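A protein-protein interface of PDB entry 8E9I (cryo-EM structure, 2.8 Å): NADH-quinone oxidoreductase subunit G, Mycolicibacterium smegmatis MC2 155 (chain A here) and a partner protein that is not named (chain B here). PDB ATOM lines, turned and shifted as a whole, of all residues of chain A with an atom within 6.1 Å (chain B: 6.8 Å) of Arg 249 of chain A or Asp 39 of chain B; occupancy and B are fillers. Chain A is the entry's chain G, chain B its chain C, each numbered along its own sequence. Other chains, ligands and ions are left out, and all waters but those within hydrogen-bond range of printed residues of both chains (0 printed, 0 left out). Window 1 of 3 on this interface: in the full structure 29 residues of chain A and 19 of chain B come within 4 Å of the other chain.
O of Gln 211 of chain A is in hydrogen-bond range of N of Ser 41 of chain B, at 2.9 Å.
NH1 of Arg 249 of chain A sits close to N of Asp 39 of chain B (3.4 Å).
N of Arg 235 of chain B is in hydrogen-bond range of O of Leu 232 of chain A (2.8 Å).
The guanidinium group (NH1) of Arg 249 of chain A lies close to the backbone carbonyl oxygen (O) of Gly 38 of chain B, at 3.5 Å.
NH2 of Arg 235 of chain B lies close to NH1 of Arg 249 of chain A (2.9 Å).
The side-chain amide oxygen (OD1) of Asn 34 of chain B sits at hydrogen-bond distance from the guanidinium group (NH2) of Arg 235 of chain B, at 2.7 Å.
OH of Tyr 237 of chain B is in hydrogen-bond range of NE of Arg 235 of chain B (2.6 Å).
The guanidinium group (NH2) of Arg 249 of chain A is in salt-bridge range of the side-chain carboxylate (OD2) of Asp 251 of chain A, at 2.5 Å.
OE1 of Gln 211 of chain A is in hydrogen-bond range of N of Ala 262 of chain A (2.6 Å).
OD1 of Asp 251 of chain A sits at hydrogen-bond distance from OG of Ser 234 of chain A (2.5 Å).
The backbone NH (N) of Arg 249 of chain A sits at hydrogen-bond distance from the backbone carbonyl oxygen (O) of Leu 261 of chain A, at 2.9 Å.
Among the printed residues, pairs that only touch across the chains: Lys 119 of chain A with Thr 40 of chain B (3.6 Å), Glu 122 of chain A with Asp 39 of chain B (3.9 Å), Glu 122 of chain A with Thr 40 of chain B (3.8 Å), Gln 211 of chain A with Asp 39 of chain B (3.9 Å), Gln 211 of chain A with Thr 40 of chain B (3.4 Å), Ser 234 of chain A with Arg 235 of chain B (3.6 Å), Arg 249 of chain A with Thr 37 of chain B (3.5 Å), Leu 261 of chain A with Asp 39 of chain B (3.8 Å) and Gly 263 of chain A with Thr 37 of chain B (3.7 Å).
Printed residues of chain B within 4 Å of Gln 211 of chain A: Asp 39 (3.9 Å), Thr 40 (3.4 Å) and Ser 41 (2.9 Å).
Of the printed residues of chain B, Ser 234 of chain A touches Arg 235.
Of chain B, only Thr 37 (3.5 Å), Gly 38 (3.3 Å), Asp 39 (3.4 Å) and Arg 235 (2.9 Å) come within 4 Å of Arg 249 of chain A.
Of the printed residues of chain B, Leu 261 of chain A touches Asp 39 (3.8 Å).
Of the printed residues of chain A, Gly 38 of chain B touches Arg 249.
Of chain A, only Glu 122 (3.9 Å), Gln 211 (3.9 Å), Arg 249 (3.4 Å) and Leu 261 (3.8 Å) come within 4 Å of Asp 39 of chain B.
The nearest printed residue of chain A that does not touch Thr 37 of chain B is Ala 262 of chain A (5.7 Å).
Hydrophobic or aromatic side chains of chain A within 4 Å of the printed part of chain B: Leu 261.
Along chain B the printed residues that touch a printed residue of chain A span positions 37 to 235.
Among the printed residues, no Asp or Glu carboxylate lies within 4 Å of a Lys or Arg side-chain nitrogen of the other chain.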
ATOM      1  N   LYS A 119     -13.453  -2.380   0.258  1.00  0.00           N
ATOM      2  CA  LYS A 119     -14.284  -2.158   1.428  1.00  0.00           C
ATOM      3  C   LYS A 119     -15.681  -1.667   1.068  1.00  0.00           C
ATOM      4  O   LYS A 119     -16.540  -1.607   1.951  1.00  0.00           O
ATOM      5  CB  LYS A 119     -13.594  -1.170   2.366  1.00  0.00           C
ATOM      6  CG  LYS A 119     -14.229  -1.073   3.732  1.00  0.00           C
ATOM      7  CD  LYS A 119     -13.952  -2.273   4.614  1.00  0.00           C
ATOM      8  CE  LYS A 119     -12.609  -2.188   5.291  1.00  0.00           C
ATOM      9  NZ  LYS A 119     -12.480  -3.215   6.354  1.00  0.00           N
ATOM     10  N   GLU A 122     -19.105  -2.746   2.765  1.00  0.00           N
ATOM     11  CA  GLU A 122     -18.816  -3.030   4.161  1.00  0.00           C
ATOM     12  C   GLU A 122     -18.010  -1.927   4.824  1.00  0.00           C
ATOM     13  O   GLU A 122     -17.379  -2.183   5.853  1.00  0.00           O
ATOM     14  CB  GLU A 122     -18.062  -4.352   4.285  1.00  0.00           C
ATOM     15  N   VAL A 210      -6.198  -5.738   8.382  1.00  0.00           N
ATOM     16  CA  VAL A 210      -7.154  -5.661   7.285  1.00  0.00           C
ATOM     17  C   VAL A 210      -8.571  -5.655   7.834  1.00  0.00           C
ATOM     18  O   VAL A 210      -9.438  -4.916   7.355  1.00  0.00           O
ATOM     19  CB  VAL A 210      -6.932  -6.823   6.305  1.00  0.00           C
ATOM     20  CG1 VAL A 210      -7.967  -6.791   5.204  1.00  0.00           C
ATOM     21  CG2 VAL A 210      -5.539  -6.759   5.727  1.00  0.00           C
ATOM     22  N   GLN A 211      -8.829  -6.471   8.852  1.00  0.00           N
ATOM     23  CA  GLN A 211     -10.163  -6.510   9.428  1.00  0.00           C
ATOM     24  C   GLN A 211     -10.405  -5.367  10.396  1.00  0.00           C
ATOM     25  O   GLN A 211     -11.559  -5.093  10.737  1.00  0.00           O
ATOM     26  CB  GLN A 211     -10.391  -7.837  10.142  1.00  0.00           C
ATOM     27  CG  GLN A 211     -11.841  -8.097  10.449  1.00  0.00           C
ATOM     28  CD  GLN A 211     -12.074  -9.483  10.976  1.00  0.00           C
ATOM     29  OE1 GLN A 211     -11.279 -10.389  10.738  1.00  0.00           O
ATOM     30  NE2 GLN A 211     -13.167  -9.664  11.700  1.00  0.00           N
ATOM     31  N   LEU A 232     -21.167 -12.615  -1.339  1.00  0.00           N
ATOM     32  CA  LEU A 232     -20.535 -13.576  -0.445  1.00  0.00           C
ATOM     33  C   LEU A 232     -21.580 -14.404   0.284  1.00  0.00           C
ATOM     34  O   LEU A 232     -22.497 -13.854   0.900  1.00  0.00           O
ATOM     35  CB  LEU A 232     -19.668 -12.851   0.578  1.00  0.00           C
ATOM     36  CG  LEU A 232     -18.246 -12.450   0.218  1.00  0.00           C
ATOM     37  CD1 LEU A 232     -18.238 -11.502  -0.933  1.00  0.00           C
ATOM     38  CD2 LEU A 232     -17.620 -11.782   1.416  1.00  0.00           C
ATOM     39  N   SER A 234     -21.762 -16.172   3.587  1.00  0.00           N
ATOM     40  CA  SER A 234     -20.994 -15.997   4.815  1.00  0.00           C
ATOM     41  C   SER A 234     -21.514 -16.996   5.835  1.00  0.00           C
ATOM     42  O   SER A 234     -22.729 -17.131   6.002  1.00  0.00           O
ATOM     43  CB  SER A 234     -21.115 -14.566   5.331  1.00  0.00           C
ATOM     44  OG  SER A 234     -20.099 -14.270   6.263  1.00  0.00           O
ATOM     45  N   SER A 235     -20.604 -17.709   6.499  1.00  0.00           N
ATOM     46  CA  SER A 235     -20.995 -18.692   7.495  1.00  0.00           C
ATOM     47  C   SER A 235     -20.069 -18.632   8.699  1.00  0.00           C
ATOM     48  O   SER A 235     -18.876 -18.355   8.549  1.00  0.00           O
ATOM     49  CB  SER A 235     -20.965 -20.101   6.900  1.00  0.00           C
ATOM     50  OG  SER A 235     -21.713 -20.157   5.701  1.00  0.00           O
ATOM     51  N   PRO A 236     -20.575 -18.874   9.905  1.00  0.00           N
ATOM     52  CA  PRO A 236     -19.671 -19.058  11.042  1.00  0.00           C
ATOM     53  C   PRO A 236     -18.855 -20.326  10.866  1.00  0.00           C
ATOM     54  O   PRO A 236     -19.267 -21.265  10.186  1.00  0.00           O
ATOM     55  CB  PRO A 236     -20.617 -19.158  12.241  1.00  0.00           C
ATOM     56  CG  PRO A 236     -21.869 -18.525  11.790  1.00  0.00           C
ATOM     57  CD  PRO A 236     -21.979 -18.841  10.338  1.00  0.00           C
ATOM     58  N   SER A 237     -17.682 -20.347  11.483  1.00  0.00           N
ATOM     59  CA  SER A 237     -16.784 -21.478  11.327  1.00  0.00           C
ATOM     60  C   SER A 237     -15.771 -21.455  12.456  1.00  0.00           C
ATOM     61  O   SER A 237     -15.722 -20.524  13.259  1.00  0.00           O
ATOM     62  CB  SER A 237     -16.082 -21.445   9.971  1.00  0.00           C
ATOM     63  OG  SER A 237     -16.989 -21.717   8.924  1.00  0.00           O
ATOM     64  N   ALA A 247     -13.279 -18.604  16.772  1.00  0.00           N
ATOM     65  CA  ALA A 247     -14.426 -18.338  15.929  1.00  0.00           C
ATOM     66  C   ALA A 247     -13.978 -17.544  14.714  1.00  0.00           C
ATOM     67  O   ALA A 247     -13.197 -16.598  14.819  1.00  0.00           O
ATOM     68  CB  ALA A 247     -15.495 -17.571  16.699  1.00  0.00           C
ATOM     69  N   GLN A 248     -14.467 -17.949  13.548  1.00  0.00           N
ATOM     70  CA  GLN A 248     -14.129 -17.282  12.303  1.00  0.00           C
ATOM     71  C   GLN A 248     -15.383 -17.174  11.460  1.00  0.00           C
ATOM     72  O   GLN A 248     -16.395 -17.817  11.737  1.00  0.00           O
ATOM     73  CB  GLN A 248     -13.045 -18.035  11.537  1.00  0.00           C
ATOM     74  CG  GLN A 248     -11.651 -17.812  12.054  1.00  0.00           C
ATOM     75  CD  GLN A 248     -10.612 -18.335  11.098  1.00  0.00           C
ATOM     76  OE1 GLN A 248     -10.784 -19.396  10.505  1.00  0.00           O
ATOM     77  NE2 GLN A 248      -9.527 -17.597  10.942  1.00  0.00           N
ATOM     78  N   ARG A 249     -15.310 -16.346  10.433  1.00  0.00           N
ATOM     79  CA  ARG A 249     -16.397 -16.174   9.482  1.00  0.00           C
ATOM     80  C   ARG A 249     -15.860 -16.485   8.098  1.00  0.00           C
ATOM     81  O   ARG A 249     -15.052 -15.724   7.561  1.00  0.00           O
ATOM     82  CB  ARG A 249     -16.959 -14.757   9.533  1.00  0.00           C
ATOM     83  CG  ARG A 249     -18.377 -14.652   9.023  1.00  0.00           C
ATOM     84  CD  ARG A 249     -18.791 -13.214   8.812  1.00  0.00           C
ATOM     85  NE  ARG A 249     -18.287 -12.687   7.552  1.00  0.00           N
ATOM     86  CZ  ARG A 249     -18.281 -11.403   7.223  1.00  0.00           C
ATOM     87  NH1 ARG A 249     -18.737 -10.476   8.046  1.00  0.00           N
ATOM     88  NH2 ARG A 249     -17.813 -11.042   6.034  1.00  0.00           N
ATOM     89  N   THR A 250     -16.293 -17.606   7.537  1.00  0.00           N
ATOM     90  CA  THR A 250     -15.853 -18.016   6.215  1.00  0.00           C
ATOM     91  C   THR A 250     -16.760 -17.401   5.165  1.00  0.00           C
ATOM     92  O   THR A 250     -17.983 -17.552   5.225  1.00  0.00           O
ATOM     93  CB  THR A 250     -15.870 -19.537   6.101  1.00  0.00           C
ATOM     94  OG1 THR A 250     -14.977 -20.098   7.068  1.00  0.00           O
ATOM     95  CG2 THR A 250     -15.455 -19.976   4.713  1.00  0.00           C
ATOM     96  N   ASP A 251     -16.160 -16.706   4.205  1.00  0.00           N
ATOM     97  CA  ASP A 251     -16.884 -16.072   3.116  1.00  0.00           C
ATOM     98  C   ASP A 251     -16.476 -16.748   1.820  1.00  0.00           C
ATOM     99  O   ASP A 251     -15.286 -16.804   1.497  1.00  0.00           O
ATOM    100  CB  ASP A 251     -16.580 -14.578   3.058  1.00  0.00           C
ATOM    101  CG  ASP A 251     -17.229 -13.810   4.181  1.00  0.00           C
ATOM    102  OD1 ASP A 251     -18.055 -14.398   4.903  1.00  0.00           O
ATOM    103  OD2 ASP A 251     -16.917 -12.616   4.343  1.00  0.00           O
ATOM    104  N   ARG A 259     -12.247 -15.564   1.923  1.00  0.00           N
ATOM    105  CA  ARG A 259     -11.579 -15.042   3.103  1.00  0.00           C
ATOM    106  C   ARG A 259     -12.194 -15.663   4.344  1.00  0.00           C
ATOM    107  O   ARG A 259     -13.280 -16.247   4.304  1.00  0.00           O
ATOM    108  CB  ARG A 259     -11.666 -13.517   3.160  1.00  0.00           C
ATOM    109  CG  ARG A 259     -13.078 -12.984   3.190  1.00  0.00           C
ATOM    110  CD  ARG A 259     -13.099 -11.495   3.415  1.00  0.00           C
ATOM    111  NE  ARG A 259     -14.461 -10.995   3.530  1.00  0.00           N
ATOM    112  CZ  ARG A 259     -14.797  -9.715   3.480  1.00  0.00           C
ATOM    113  NH1 ARG A 259     -13.887  -8.766   3.345  1.00  0.00           N
ATOM    114  NH2 ARG A 259     -16.078  -9.376   3.586  1.00  0.00           N
ATOM    115  N   ARG A 260     -11.473 -15.536   5.450  1.00  0.00           N
ATOM    116  CA  ARG A 260     -11.920 -16.033   6.741  1.00  0.00           C
ATOM    117  C   ARG A 260     -11.661 -14.957   7.781  1.00  0.00           C
ATOM    118  O   ARG A 260     -10.566 -14.883   8.343  1.00  0.00           O
ATOM    119  CB  ARG A 260     -11.205 -17.333   7.100  1.00  0.00           C
ATOM    120  CG  ARG A 260     -11.277 -18.377   6.005  1.00  0.00           C
ATOM    121  CD  ARG A 260     -11.171 -19.779   6.564  1.00  0.00           C
ATOM    122  NE  ARG A 260      -9.859 -20.048   7.135  1.00  0.00           N
ATOM    123  CZ  ARG A 260      -9.372 -21.262   7.354  1.00  0.00           C
ATOM    124  NH1 ARG A 260     -10.076 -22.348   7.090  1.00  0.00           N
ATOM    125  NH2 ARG A 260      -8.149 -21.388   7.856  1.00  0.00           N
ATOM    126  N   LEU A 261     -12.667 -14.131   8.031  1.00  0.00           N
ATOM    127  CA  LEU A 261     -12.540 -13.053   8.993  1.00  0.00           C
ATOM    128  C   LEU A 261     -12.559 -13.600  10.415  1.00  0.00           C
ATOM    129  O   LEU A 261     -12.946 -14.740  10.663  1.00  0.00           O
ATOM    130  CB  LEU A 261     -13.660 -12.037   8.797  1.00  0.00           C
ATOM    131  CG  LEU A 261     -13.682 -11.362   7.429  1.00  0.00           C
ATOM    132  CD1 LEU A 261     -14.802 -10.356   7.348  1.00  0.00           C
ATOM    133  CD2 LEU A 261     -12.362 -10.679   7.155  1.00  0.00           C
ATOM    134  N   ALA A 262     -12.150 -12.757  11.360  1.00  0.00           N
ATOM    135  CA  ALA A 262     -11.910 -13.195  12.728  1.00  0.00           C
ATOM    136  C   ALA A 262     -13.174 -13.506  13.509  1.00  0.00           C
ATOM    137  O   ALA A 262     -13.068 -14.117  14.574  1.00  0.00           O
ATOM    138  CB  ALA A 262     -11.110 -12.133  13.474  1.00  0.00           C
ATOM    139  N   GLY A 263     -14.348 -13.116  13.041  1.00  0.00           N
ATOM    140  CA  GLY A 263     -15.483 -13.430  13.872  1.00  0.00           C
ATOM    141  C   GLY A 263     -15.372 -12.705  15.204  1.00  0.00           C
ATOM    142  O   GLY A 263     -14.571 -11.789  15.385  1.00  0.00           O
ATOM    143  N   ASN B  34     -25.288  -5.521  10.651  1.00  0.00           N
ATOM    144  CA  ASN B  34     -24.731  -6.858  10.530  1.00  0.00           C
ATOM    145  C   ASN B  34     -25.650  -7.862  11.204  1.00  0.00           C
ATOM    146  O   ASN B  34     -26.065  -7.671  12.349  1.00  0.00           O
ATOM    147  CB  ASN B  34     -23.342  -6.925  11.161  1.00  0.00           C
ATOM    148  CG  ASN B  34     -22.261  -6.443  10.229  1.00  0.00           C
ATOM    149  OD1 ASN B  34     -22.041  -7.023   9.168  1.00  0.00           O
ATOM    150  ND2 ASN B  34     -21.557  -5.394  10.629  1.00  0.00           N
ATOM    151  N   ASP B  36     -24.514 -10.866  11.670  1.00  0.00           N
ATOM    152  CA  ASP B  36     -23.561 -11.738  12.345  1.00  0.00           C
ATOM    153  C   ASP B  36     -22.308 -10.947  12.692  1.00  0.00           C
ATOM    154  O   ASP B  36     -22.342  -9.714  12.710  1.00  0.00           O
ATOM    155  CB  ASP B  36     -23.237 -12.961  11.481  1.00  0.00           C
ATOM    156  CG  ASP B  36     -22.759 -12.592  10.096  1.00  0.00           C
ATOM    157  OD1 ASP B  36     -22.353 -11.433   9.887  1.00  0.00           O
ATOM    158  OD2 ASP B  36     -22.787 -13.472   9.210  1.00  0.00           O
ATOM    159  N   THR B  37     -21.206 -11.644  12.987  1.00  0.00           N
ATOM    160  CA  THR B  37     -20.043 -11.017  13.609  1.00  0.00           C
ATOM    161  C   THR B  37     -19.677  -9.671  13.002  1.00  0.00           C
ATOM    162  O   THR B  37     -19.310  -8.756  13.745  1.00  0.00           O
ATOM    163  CB  THR B  37     -18.838 -11.949  13.524  1.00  0.00           C
ATOM    164  OG1 THR B  37     -18.527 -12.202  12.150  1.00  0.00           O
ATOM    165  CG2 THR B  37     -19.121 -13.257  14.237  1.00  0.00           C
ATOM    166  N   GLY B  38     -19.767  -9.521  11.689  1.00  0.00           N
ATOM    167  CA  GLY B  38     -19.473  -8.254  11.056  1.00  0.00           C
ATOM    168  C   GLY B  38     -18.126  -8.242  10.354  1.00  0.00           C
ATOM    169  O   GLY B  38     -17.180  -8.933  10.727  1.00  0.00           O
ATOM    170  N   ASP B  39     -18.049  -7.413   9.312  1.00  0.00           N
ATOM    171  CA  ASP B  39     -16.900  -7.420   8.420  1.00  0.00           C
ATOM    172  C   ASP B  39     -15.777  -6.503   8.882  1.00  0.00           C
ATOM    173  O   ASP B  39     -14.699  -6.523   8.283  1.00  0.00           O
ATOM    174  CB  ASP B  39     -17.339  -7.024   7.013  1.00  0.00           C
ATOM    175  N   THR B  40     -16.000  -5.698   9.916  1.00  0.00           N
ATOM    176  CA  THR B  40     -14.957  -4.876  10.515  1.00  0.00           C
ATOM    177  C   THR B  40     -14.967  -5.106  12.014  1.00  0.00           C
ATOM    178  O   THR B  40     -16.038  -5.197  12.620  1.00  0.00           O
ATOM    179  CB  THR B  40     -15.164  -3.392  10.217  1.00  0.00           C
ATOM    180  OG1 THR B  40     -15.166  -3.182   8.802  1.00  0.00           O
ATOM    181  CG2 THR B  40     -14.059  -2.567  10.841  1.00  0.00           C
ATOM    182  N   SER B  41     -13.784  -5.196  12.609  1.00  0.00           N
ATOM    183  CA  SER B  41     -13.699  -5.498  14.029  1.00  0.00           C
ATOM    184  C   SER B  41     -14.010  -4.268  14.871  1.00  0.00           C
ATOM    185  O   SER B  41     -13.747  -3.129  14.478  1.00  0.00           O
ATOM    186  CB  SER B  41     -12.312  -6.027  14.376  1.00  0.00           C
ATOM    187  OG  SER B  41     -11.949  -7.069  13.496  1.00  0.00           O
ATOM    188  N   ARG B 235     -24.838 -12.648   1.799  1.00  0.00           N
ATOM    189  CA  ARG B 235     -24.763 -11.713   2.909  1.00  0.00           C
ATOM    190  C   ARG B 235     -25.804 -10.609   2.776  1.00  0.00           C
ATOM    191  O   ARG B 235     -26.270 -10.285   1.682  1.00  0.00           O
ATOM    192  CB  ARG B 235     -23.365 -11.108   2.981  1.00  0.00           C
ATOM    193  CG  ARG B 235     -23.114 -10.331   4.243  1.00  0.00           C
ATOM    194  CD  ARG B 235     -21.638 -10.163   4.516  1.00  0.00           C
ATOM    195  NE  ARG B 235     -21.430  -9.551   5.819  1.00  0.00           N
ATOM    196  CZ  ARG B 235     -21.691 -10.149   6.971  1.00  0.00           C
ATOM    197  NH1 ARG B 235     -22.132 -11.393   7.019  1.00  0.00           N
ATOM    198  NH2 ARG B 235     -21.506  -9.481   8.105  1.00  0.00           N
ATOM    199  N   TYR B 237     -27.473  -6.890   5.117  1.00  0.00           N
ATOM    200  CA  TYR B 237     -27.360  -5.956   6.225  1.00  0.00           C
ATOM    201  C   TYR B 237     -28.703  -5.295   6.497  1.00  0.00           C
ATOM    202  O   TYR B 237     -28.767  -4.136   6.895  1.00  0.00           O
ATOM    203  CB  TYR B 237     -26.298  -4.905   5.925  1.00  0.00           C
ATOM    204  CG  TYR B 237     -24.938  -5.496   5.645  1.00  0.00           C
ATOM    205  CD1 TYR B 237     -24.588  -5.899   4.367  1.00  0.00           C
ATOM    206  CD2 TYR B 237     -24.008  -5.659   6.657  1.00  0.00           C
ATOM    207  CE1 TYR B 237     -23.355  -6.446   4.104  1.00  0.00           C
ATOM    208  CE2 TYR B 237     -22.769  -6.203   6.403  1.00  0.00           C
ATOM    209  CZ  TYR B 237     -22.448  -6.593   5.125  1.00  0.00           C
ATOM    210  OH  TYR B 237     -21.215  -7.137   4.870  1.00  0.00           O
